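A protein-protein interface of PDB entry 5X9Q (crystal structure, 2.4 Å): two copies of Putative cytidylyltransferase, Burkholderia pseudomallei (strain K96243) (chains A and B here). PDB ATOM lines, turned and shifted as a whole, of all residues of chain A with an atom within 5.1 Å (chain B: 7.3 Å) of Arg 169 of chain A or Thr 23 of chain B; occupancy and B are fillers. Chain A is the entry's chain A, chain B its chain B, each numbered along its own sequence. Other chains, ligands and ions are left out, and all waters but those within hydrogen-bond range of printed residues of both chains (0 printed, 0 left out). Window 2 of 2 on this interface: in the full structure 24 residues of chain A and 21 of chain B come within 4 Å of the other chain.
Among the printed residues, pairs that only touch across the chains: Leu 165 of chain A with Glu 18 of chain B, Arg 169 of chain A with Thr 23 of chain B, Arg 169 of chain A with Leu 21 of chain B and Leu 165 of chain A with Arg 19 of chain B.
No position is printed for both chains. Of the 8 pairs that touch across the chains among the printed residues, none has its exchanged pair printed and touching as well.
Hydrophobic or aromatic side chains of chain B within 4 Å of the printed part of chain A: Leu 21. Of the 9 printed residues of chain A, 4 touch a printed residue of chain B. Among the printed residues, 8 pairs touch across the chains. Among the printed residues, Asp or Glu carboxylates within 4 Å of a Lys or Arg side-chain nitrogen of the other chain: Arg 169 of chain A with Glu 91 of chain B.
Printed residues of chain B within 4 Å of Leu 165 of chain A: Glu 18 (2.9 Å) and Arg 19 (3.5 Å). Lys 167 of chain A touches none of the printed residues of chain B. Of chain B, only Leu 21 (3.5 Å), Thr 23 (3.5 Å) and Glu 91 (3.7 Å) come within 4 Å of Arg 169 of chain A. Gln 171 of chain A touches none of the printed residues of chain B. Of the printed residues of chain A, Glu 18 of chain B touches Thr 162 and Leu 165. Of the printed residues of chain A, Arg 19 of chain B touches Leu 165 (3.5 Å). Printed residues of chain A within 4 Å of Leu 21 of chain B: Arg 169 (3.5 Å). Of the printed residues of chain A, Thr 23 of chain B touches Arg 169 (3.5 Å) and Ser 172 (2.8 Å). Printed residues of chain A within 4 Å of Glu 91 of chain B: Arg 169. The nearest residue of chain B that does not touch Arg 169 of chain A is Glu 18 of chain B (4.1 Å). The nearest printed residue of chain A that does not touch Thr 23 of chain B is Ala 170 of chain A (5.4 Å). The nearest printed residue of chain A that does not touch Glu 18 of chain B is Arg 169 of chain A (4.1 Å).
The side-chain carboxylate of Asp 25 of chain B sits close to the side-chain hydroxyl of Ser 172 of chain A (3.2 Å). The side-chain hydroxyl (OG1) of Thr 162 of chain A sits at hydrogen-bond distance from the side-chain carboxylate (OE1) of Glu 18 of chain B, 3.1 Å away. The guanidinium group (NH2) of Arg 169 of chain A is in salt-bridge range of the side-chain carboxylate (OE2) of Glu 91 of chain B (3.7 Å). The side-chain hydroxyl of Thr 23 of chain B lies close to the side-chain hydroxyl of Ser 172 of chain A (2.9 Å).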
ATOM      1  N   THR A 162       0.538  -9.516  17.753  1.00  0.00           N
ATOM      2  CA  THR A 162       0.096  -9.132  16.413  1.00  0.00           C
ATOM      3  C   THR A 162      -0.099  -7.652  16.080  1.00  0.00           C
ATOM      4  O   THR A 162       0.414  -7.158  15.076  1.00  0.00           O
ATOM      5  CB  THR A 162      -1.201  -9.888  16.058  1.00  0.00           C
ATOM      6  OG1 THR A 162      -1.447  -9.783  14.650  1.00  0.00           O
ATOM      7  CG2 THR A 162      -2.381  -9.309  16.821  1.00  0.00           C
ATOM      8  N   LEU A 165       3.570  -5.768  15.660  1.00  0.00           N
ATOM      9  CA  LEU A 165       4.278  -6.054  14.414  1.00  0.00           C
ATOM     10  C   LEU A 165       3.703  -5.430  13.143  1.00  0.00           C
ATOM     11  O   LEU A 165       4.438  -4.894  12.313  1.00  0.00           O
ATOM     12  CB  LEU A 165       4.324  -7.564  14.165  1.00  0.00           C
ATOM     13  CG  LEU A 165       5.155  -8.388  15.149  1.00  0.00           C
ATOM     14  CD1 LEU A 165       5.089  -9.868  14.801  1.00  0.00           C
ATOM     15  CD2 LEU A 165       6.597  -7.903  15.174  1.00  0.00           C
ATOM     16  N   LYS A 166       2.385  -5.467  13.021  1.00  0.00           N
ATOM     17  CA  LYS A 166       1.687  -4.914  11.870  1.00  0.00           C
ATOM     18  C   LYS A 166       1.632  -3.398  11.966  1.00  0.00           C
ATOM     19  O   LYS A 166       1.610  -2.701  10.952  1.00  0.00           O
ATOM     20  CB  LYS A 166       0.226  -5.368  11.847  1.00  0.00           C
ATOM     21  CG  LYS A 166      -0.654  -4.575  10.895  1.00  0.00           C
ATOM     22  CD  LYS A 166      -2.127  -4.846  11.151  1.00  0.00           C
ATOM     23  CE  LYS A 166      -2.955  -4.632   9.893  1.00  0.00           C
ATOM     24  NZ  LYS A 166      -4.363  -5.081  10.071  1.00  0.00           N
ATOM     25  N   LYS A 167       1.584  -2.908  13.200  1.00  0.00           N
ATOM     26  CA  LYS A 167       1.561  -1.480  13.452  1.00  0.00           C
ATOM     27  C   LYS A 167       2.799  -0.963  12.727  1.00  0.00           C
ATOM     28  O   LYS A 167       2.761   0.056  12.076  1.00  0.00           O
ATOM     29  CB  LYS A 167       1.657  -1.206  14.962  1.00  0.00           C
ATOM     30  CG  LYS A 167       0.450  -1.657  15.790  1.00  0.00           C
ATOM     31  CD  LYS A 167       0.618  -1.378  17.290  1.00  0.00           C
ATOM     32  CE  LYS A 167      -0.600  -1.809  18.116  1.00  0.00           C
ATOM     33  NZ  LYS A 167      -0.481  -1.580  19.596  1.00  0.00           N
ATOM     34  N   VAL A 168       3.876  -1.718  12.890  1.00  0.00           N
ATOM     35  CA  VAL A 168       5.203  -1.581  12.316  1.00  0.00           C
ATOM     36  C   VAL A 168       5.090  -1.630  10.781  1.00  0.00           C
ATOM     37  O   VAL A 168       5.748  -0.889  10.090  1.00  0.00           O
ATOM     38  CB  VAL A 168       6.147  -2.690  12.852  1.00  0.00           C
ATOM     39  CG1 VAL A 168       7.512  -2.652  12.182  1.00  0.00           C
ATOM     40  CG2 VAL A 168       6.331  -2.547  14.348  1.00  0.00           C
ATOM     41  N   ARG A 169       4.210  -2.483  10.264  1.00  0.00           N
ATOM     42  CA  ARG A 169       4.011  -2.618   8.817  1.00  0.00           C
ATOM     43  C   ARG A 169       3.474  -1.339   8.191  1.00  0.00           C
ATOM     44  O   ARG A 169       4.011  -0.884   7.216  1.00  0.00           O
ATOM     45  CB  ARG A 169       3.329  -3.941   8.460  1.00  0.00           C
ATOM     46  CG  ARG A 169       4.193  -5.157   8.693  1.00  0.00           C
ATOM     47  CD  ARG A 169       3.627  -6.407   8.049  1.00  0.00           C
ATOM     48  NE  ARG A 169       2.329  -6.812   8.588  1.00  0.00           N
ATOM     49  CZ  ARG A 169       2.196  -7.576   9.664  1.00  0.00           C
ATOM     50  NH1 ARG A 169       3.276  -8.008  10.279  1.00  0.00           N
ATOM     51  NH2 ARG A 169       0.999  -7.906  10.118  1.00  0.00           N
ATOM     52  N   ALA A 170       2.421  -0.749   8.734  1.00  0.00           N
ATOM     53  CA  ALA A 170       1.924   0.517   8.183  1.00  0.00           C
ATOM     54  C   ALA A 170       2.891   1.642   7.935  1.00  0.00           C
ATOM     55  O   ALA A 170       2.853   2.338   6.921  1.00  0.00           O
ATOM     56  CB  ALA A 170       0.744   1.007   9.011  1.00  0.00           C
ATOM     57  N   GLN A 171       3.759   1.793   8.909  1.00  0.00           N
ATOM     58  CA  GLN A 171       4.790   2.802   8.950  1.00  0.00           C
ATOM     59  C   GLN A 171       5.433   2.866   7.594  1.00  0.00           C
ATOM     60  O   GLN A 171       5.552   3.949   7.022  1.00  0.00           O
ATOM     61  CB  GLN A 171       5.833   2.463  10.016  1.00  0.00           C
ATOM     62  CG  GLN A 171       6.214   3.632  10.907  1.00  0.00           C
ATOM     63  CD  GLN A 171       5.067   4.093  11.784  1.00  0.00           C
ATOM     64  OE1 GLN A 171       4.441   3.293  12.480  1.00  0.00           O
ATOM     65  NE2 GLN A 171       4.784   5.391  11.756  1.00  0.00           N
ATOM     66  N   SER A 172       5.853   1.727   7.045  1.00  0.00           N
ATOM     67  CA  SER A 172       6.447   1.874   5.722  1.00  0.00           C
ATOM     68  C   SER A 172       5.546   2.665   4.754  1.00  0.00           C
ATOM     69  O   SER A 172       5.611   2.488   3.531  1.00  0.00           O
ATOM     70  CB  SER A 172       6.834   0.517   5.151  1.00  0.00           C
ATOM     71  OG  SER A 172       7.315   0.626   3.820  1.00  0.00           O
ATOM     72  N   GLU B  18       5.621 -13.768  13.209  1.00  0.00           N
ATOM     73  CA  GLU B  18       5.181 -12.593  12.465  1.00  0.00           C
ATOM     74  C   GLU B  18       6.292 -11.561  12.316  1.00  0.00           C
ATOM     75  O   GLU B  18       6.131 -10.562  11.613  1.00  0.00           O
ATOM     76  CB  GLU B  18       3.963 -11.959  13.142  1.00  0.00           C
ATOM     77  CG  GLU B  18       2.708 -12.816  13.093  1.00  0.00           C
ATOM     78  CD  GLU B  18       1.438 -11.991  13.154  1.00  0.00           C
ATOM     79  OE1 GLU B  18       1.154 -11.411  14.224  1.00  0.00           O
ATOM     80  OE2 GLU B  18       0.722 -11.924  12.133  1.00  0.00           O
ATOM     81  N   ARG B  19       7.418 -11.804  12.978  1.00  0.00           N
ATOM     82  CA  ARG B  19       8.543 -10.894  12.914  1.00  0.00           C
ATOM     83  C   ARG B  19       9.043 -10.912  11.472  1.00  0.00           C
ATOM     84  O   ARG B  19       9.678  -9.962  11.014  1.00  0.00           O
ATOM     85  CB  ARG B  19       9.652 -11.336  13.868  1.00  0.00           C
ATOM     86  CG  ARG B  19      10.303 -12.658  13.494  1.00  0.00           C
ATOM     87  CD  ARG B  19      11.325 -13.085  14.536  1.00  0.00           C
ATOM     88  NE  ARG B  19      11.993 -14.330  14.168  1.00  0.00           N
ATOM     89  CZ  ARG B  19      11.492 -15.541  14.390  1.00  0.00           C
ATOM     90  NH1 ARG B  19      10.313 -15.674  14.983  1.00  0.00           N
ATOM     91  NH2 ARG B  19      12.171 -16.619  14.022  1.00  0.00           N
ATOM     92  N   LYS B  20       8.750 -11.999  10.757  1.00  0.00           N
ATOM     93  CA  LYS B  20       9.158 -12.119   9.372  1.00  0.00           C
ATOM     94  C   LYS B  20       8.351 -11.386   8.306  1.00  0.00           C
ATOM     95  O   LYS B  20       8.838 -11.190   7.203  1.00  0.00           O
ATOM     96  CB  LYS B  20       9.201 -13.619   9.064  1.00  0.00           C
ATOM     97  CG  LYS B  20      10.031 -14.446  10.043  1.00  0.00           C
ATOM     98  CD  LYS B  20      10.058 -15.912   9.603  1.00  0.00           C
ATOM     99  CE  LYS B  20      10.665 -16.792  10.665  1.00  0.00           C
ATOM    100  NZ  LYS B  20      10.620 -18.222  10.211  1.00  0.00           N
ATOM    101  N   LEU B  21       7.130 -10.976   8.634  1.00  0.00           N
ATOM    102  CA  LEU B  21       6.303 -10.247   7.680  1.00  0.00           C
ATOM    103  C   LEU B  21       6.787  -8.802   7.640  1.00  0.00           C
ATOM    104  O   LEU B  21       6.687  -8.086   8.637  1.00  0.00           O
ATOM    105  CB  LEU B  21       4.831 -10.304   8.088  1.00  0.00           C
ATOM    106  CG  LEU B  21       4.234 -11.700   8.277  1.00  0.00           C
ATOM    107  CD1 LEU B  21       2.924 -11.624   9.047  1.00  0.00           C
ATOM    108  CD2 LEU B  21       4.032 -12.385   6.934  1.00  0.00           C
ATOM    109  N   ILE B  22       7.318  -8.370   6.499  1.00  0.00           N
ATOM    110  CA  ILE B  22       7.825  -7.015   6.395  1.00  0.00           C
ATOM    111  C   ILE B  22       7.582  -6.396   5.034  1.00  0.00           C
ATOM    112  O   ILE B  22       7.436  -7.093   4.030  1.00  0.00           O
ATOM    113  CB  ILE B  22       9.334  -6.955   6.703  1.00  0.00           C
ATOM    114  CG1 ILE B  22       9.823  -5.506   6.697  1.00  0.00           C
ATOM    115  CG2 ILE B  22      10.116  -7.791   5.701  1.00  0.00           C
ATOM    116  CD1 ILE B  22      11.252  -5.341   7.167  1.00  0.00           C
ATOM    117  N   THR B  23       7.530  -5.069   5.007  1.00  0.00           N
ATOM    118  CA  THR B  23       7.296  -4.336   3.769  1.00  0.00           C
ATOM    119  C   THR B  23       8.573  -4.189   2.950  1.00  0.00           C
ATOM    120  O   THR B  23       9.679  -4.263   3.486  1.00  0.00           O
ATOM    121  CB  THR B  23       6.712  -2.936   4.046  1.00  0.00           C
ATOM    122  OG1 THR B  23       7.700  -2.125   4.694  1.00  0.00           O
ATOM    123  CG2 THR B  23       5.481  -3.038   4.933  1.00  0.00           C
ATOM    124  N   ARG B  24       8.408  -3.980   1.649  1.00  0.00           N
ATOM    125  CA  ARG B  24       9.535  -3.820   0.747  1.00  0.00           C
ATOM    126  C   ARG B  24      10.551  -2.761   1.235  1.00  0.00           C
ATOM    127  O   ARG B  24      11.772  -2.988   1.247  1.00  0.00           O
ATOM    128  CB  ARG B  24       9.013  -3.446  -0.632  1.00  0.00           C
ATOM    129  CG  ARG B  24      10.096  -3.034  -1.610  1.00  0.00           C
ATOM    130  CD  ARG B  24       9.449  -2.583  -2.897  1.00  0.00           C
ATOM    131  NE  ARG B  24       8.337  -3.448  -3.280  1.00  0.00           N
ATOM    132  CZ  ARG B  24       7.765  -3.433  -4.483  1.00  0.00           C
ATOM    133  NH1 ARG B  24       8.213  -2.596  -5.414  1.00  0.00           N
ATOM    134  NH2 ARG B  24       6.746  -4.249  -4.754  1.00  0.00           N
ATOM    135  N   ASP B  25      10.053  -1.617   1.680  1.00  0.00           N
ATOM    136  CA  ASP B  25      10.943  -0.522   2.057  1.00  0.00           C
ATOM    137  C   ASP B  25      11.815  -0.873   3.250  1.00  0.00           C
ATOM    138  O   ASP B  25      13.030  -0.685   3.227  1.00  0.00           O
ATOM    139  CB  ASP B  25      10.114   0.716   2.367  1.00  0.00           C
ATOM    140  CG  ASP B  25       9.610   1.408   1.103  1.00  0.00           C
ATOM    141  OD1 ASP B  25      10.288   1.318   0.046  1.00  0.00           O
ATOM    142  OD2 ASP B  25       8.513   2.013   1.164  1.00  0.00           O
ATOM    143  N   ALA B  26      11.195  -1.424   4.289  1.00  0.00           N
ATOM    144  CA  ALA B  26      11.940  -1.808   5.481  1.00  0.00           C
ATOM    145  C   ALA B  26      12.947  -2.922   5.188  1.00  0.00           C
ATOM    146  O   ALA B  26      14.045  -2.913   5.741  1.00  0.00           O
ATOM    147  CB  ALA B  26      10.988  -2.225   6.589  1.00  0.00           C
ATOM    148  N   LEU B  27      12.574  -3.888   4.351  1.00  0.00           N
ATOM    149  CA  LEU B  27      13.484  -4.984   4.020  1.00  0.00           C
ATOM    150  C   LEU B  27      14.658  -4.467   3.204  1.00  0.00           C
ATOM    151  O   LEU B  27      15.821  -4.847   3.447  1.00  0.00           O
ATOM    152  CB  LEU B  27      12.747  -6.080   3.250  1.00  0.00           C
ATOM    153  CG  LEU B  27      13.523  -7.327   2.814  1.00  0.00           C
ATOM    154  CD1 LEU B  27      14.164  -8.055   3.986  1.00  0.00           C
ATOM    155  CD2 LEU B  27      12.597  -8.268   2.057  1.00  0.00           C
ATOM    156  N   ALA B  28      14.358  -3.575   2.251  1.00  0.00           N
ATOM    157  CA  ALA B  28      15.396  -2.968   1.419  1.00  0.00           C
ATOM    158  C   ALA B  28      16.408  -2.178   2.260  1.00  0.00           C
ATOM    159  O   ALA B  28      17.618  -2.268   2.048  1.00  0.00           O
ATOM    160  CB  ALA B  28      14.762  -2.067   0.366  1.00  0.00           C
ATOM    161  N   ALA B  29      15.914  -1.444   3.245  1.00  0.00           N
ATOM    162  CA  ALA B  29      16.791  -0.701   4.145  1.00  0.00           C
ATOM    163  C   ALA B  29      17.642  -1.650   4.991  1.00  0.00           C
ATOM    164  O   ALA B  29      18.758  -1.323   5.398  1.00  0.00           O
ATOM    165  CB  ALA B  29      15.971   0.219   5.044  1.00  0.00           C
ATOM    166  N   GLU B  91      -2.669 -11.845   3.677  1.00  0.00           N
ATOM    167  CA  GLU B  91      -2.014 -11.877   4.981  1.00  0.00           C
ATOM    168  C   GLU B  91      -2.007 -13.283   5.575  1.00  0.00           C
ATOM    169  O   GLU B  91      -1.090 -13.624   6.311  1.00  0.00           O
ATOM    170  CB  GLU B  91      -2.618 -10.868   5.959  1.00  0.00           C
ATOM    171  CG  GLU B  91      -1.497  -9.975   6.506  1.00  0.00           C
ATOM    172  CD  GLU B  91      -1.864  -9.179   7.742  1.00  0.00           C
ATOM    173  OE1 GLU B  91      -2.149  -9.796   8.797  1.00  0.00           O
ATOM    174  OE2 GLU B  91      -1.833  -7.928   7.662  1.00  0.00           O
ATOM    175  N   MET B  94       0.722 -15.174   3.735  1.00  0.00           N
ATOM    176  CA  MET B  94       2.024 -14.709   4.191  1.00  0.00           C
ATOM    177  C   MET B  94       2.331 -15.243   5.602  1.00  0.00           C
ATOM    178  O   MET B  94       3.459 -15.668   5.890  1.00  0.00           O
ATOM    179  CB  MET B  94       2.084 -13.185   4.179  1.00  0.00           C
ATOM    180  CG  MET B  94       2.068 -12.558   2.802  1.00  0.00           C
ATOM    181  SD  MET B  94       2.069 -10.742   2.903  1.00  0.00           S
ATOM    182  CE  MET B  94       3.736 -10.398   3.474  1.00  0.00           C
ATOM    183  N   VAL B 106       9.038 -12.603   4.625  1.00  0.00           N
ATOM    184  CA  VAL B 106       7.916 -12.714   3.692  1.00  0.00           C
ATOM    185  C   VAL B 106       7.442 -11.305   3.320  1.00  0.00           C
ATOM    186  O   VAL B 106       7.138 -10.501   4.216  1.00  0.00           O
ATOM    187  CB  VAL B 106       6.757 -13.527   4.291  1.00  0.00           C
ATOM    188  CG1 VAL B 106       5.686 -13.772   3.249  1.00  0.00           C
ATOM    189  CG2 VAL B 106       7.265 -14.859   4.858  1.00  0.00           C
ATOM    190  N   VAL B 107       7.505 -11.013   2.075  1.00  0.00           N
ATOM    191  CA  VAL B 107       7.077  -9.696   1.561  1.00  0.00           C
ATOM    192  C   VAL B 107       5.960  -9.844   0.531  1.00  0.00           C
ATOM    193  O   VAL B 107       6.049 -10.682  -0.376  1.00  0.00           O
ATOM    194  CB  VAL B 107       8.213  -8.927   0.827  1.00  0.00           C
ATOM    195  CG1 VAL B 107       8.016  -7.401   0.950  1.00  0.00           C
ATOM    196  CG2 VAL B 107       9.550  -9.288   1.371  1.00  0.00           C
ATOM    197  N   GLY B 108       4.935  -8.998   0.583  1.00  0.00           N
ATOM    198  CA  GLY B 108       3.877  -9.060  -0.420  1.00  0.00           C
ATOM    199  C   GLY B 108       4.053  -7.970  -1.476  1.00  0.00           C
ATOM    200  O   GLY B 108       4.388  -6.840  -1.121  1.00  0.00           O
ATOM    201  N   LEU B 117      10.020  -5.766  -7.019  1.00  0.00           N
ATOM    202  CA  LEU B 117      10.358  -6.218  -5.655  1.00  0.00           C
ATOM    203  C   LEU B 117      11.791  -6.748  -5.628  1.00  0.00           C
ATOM    204  O   LEU B 117      12.583  -6.395  -4.745  1.00  0.00           O
ATOM    205  CB  LEU B 117       9.385  -7.290  -5.148  1.00  0.00           C
ATOM    206  CG  LEU B 117       9.753  -7.994  -3.836  1.00  0.00           C
ATOM    207  CD1 LEU B 117       9.914  -7.030  -2.663  1.00  0.00           C
ATOM    208  CD2 LEU B 117       8.713  -9.071  -3.517  1.00  0.00           C
ATOM    209  N   VAL B 121      14.818  -5.556  -3.325  1.00  0.00           N
ATOM    210  CA  VAL B 121      15.436  -6.518  -2.430  1.00  0.00           C
ATOM    211  C   VAL B 121      16.867  -6.858  -2.845  1.00  0.00           C
ATOM    212  O   VAL B 121      17.714  -7.087  -1.980  1.00  0.00           O
ATOM    213  CB  VAL B 121      14.615  -7.819  -2.349  1.00  0.00           C
ATOM    214  CG1 VAL B 121      15.344  -8.853  -1.506  1.00  0.00           C
ATOM    215  CG2 VAL B 121      13.231  -7.538  -1.785  1.00  0.00           C
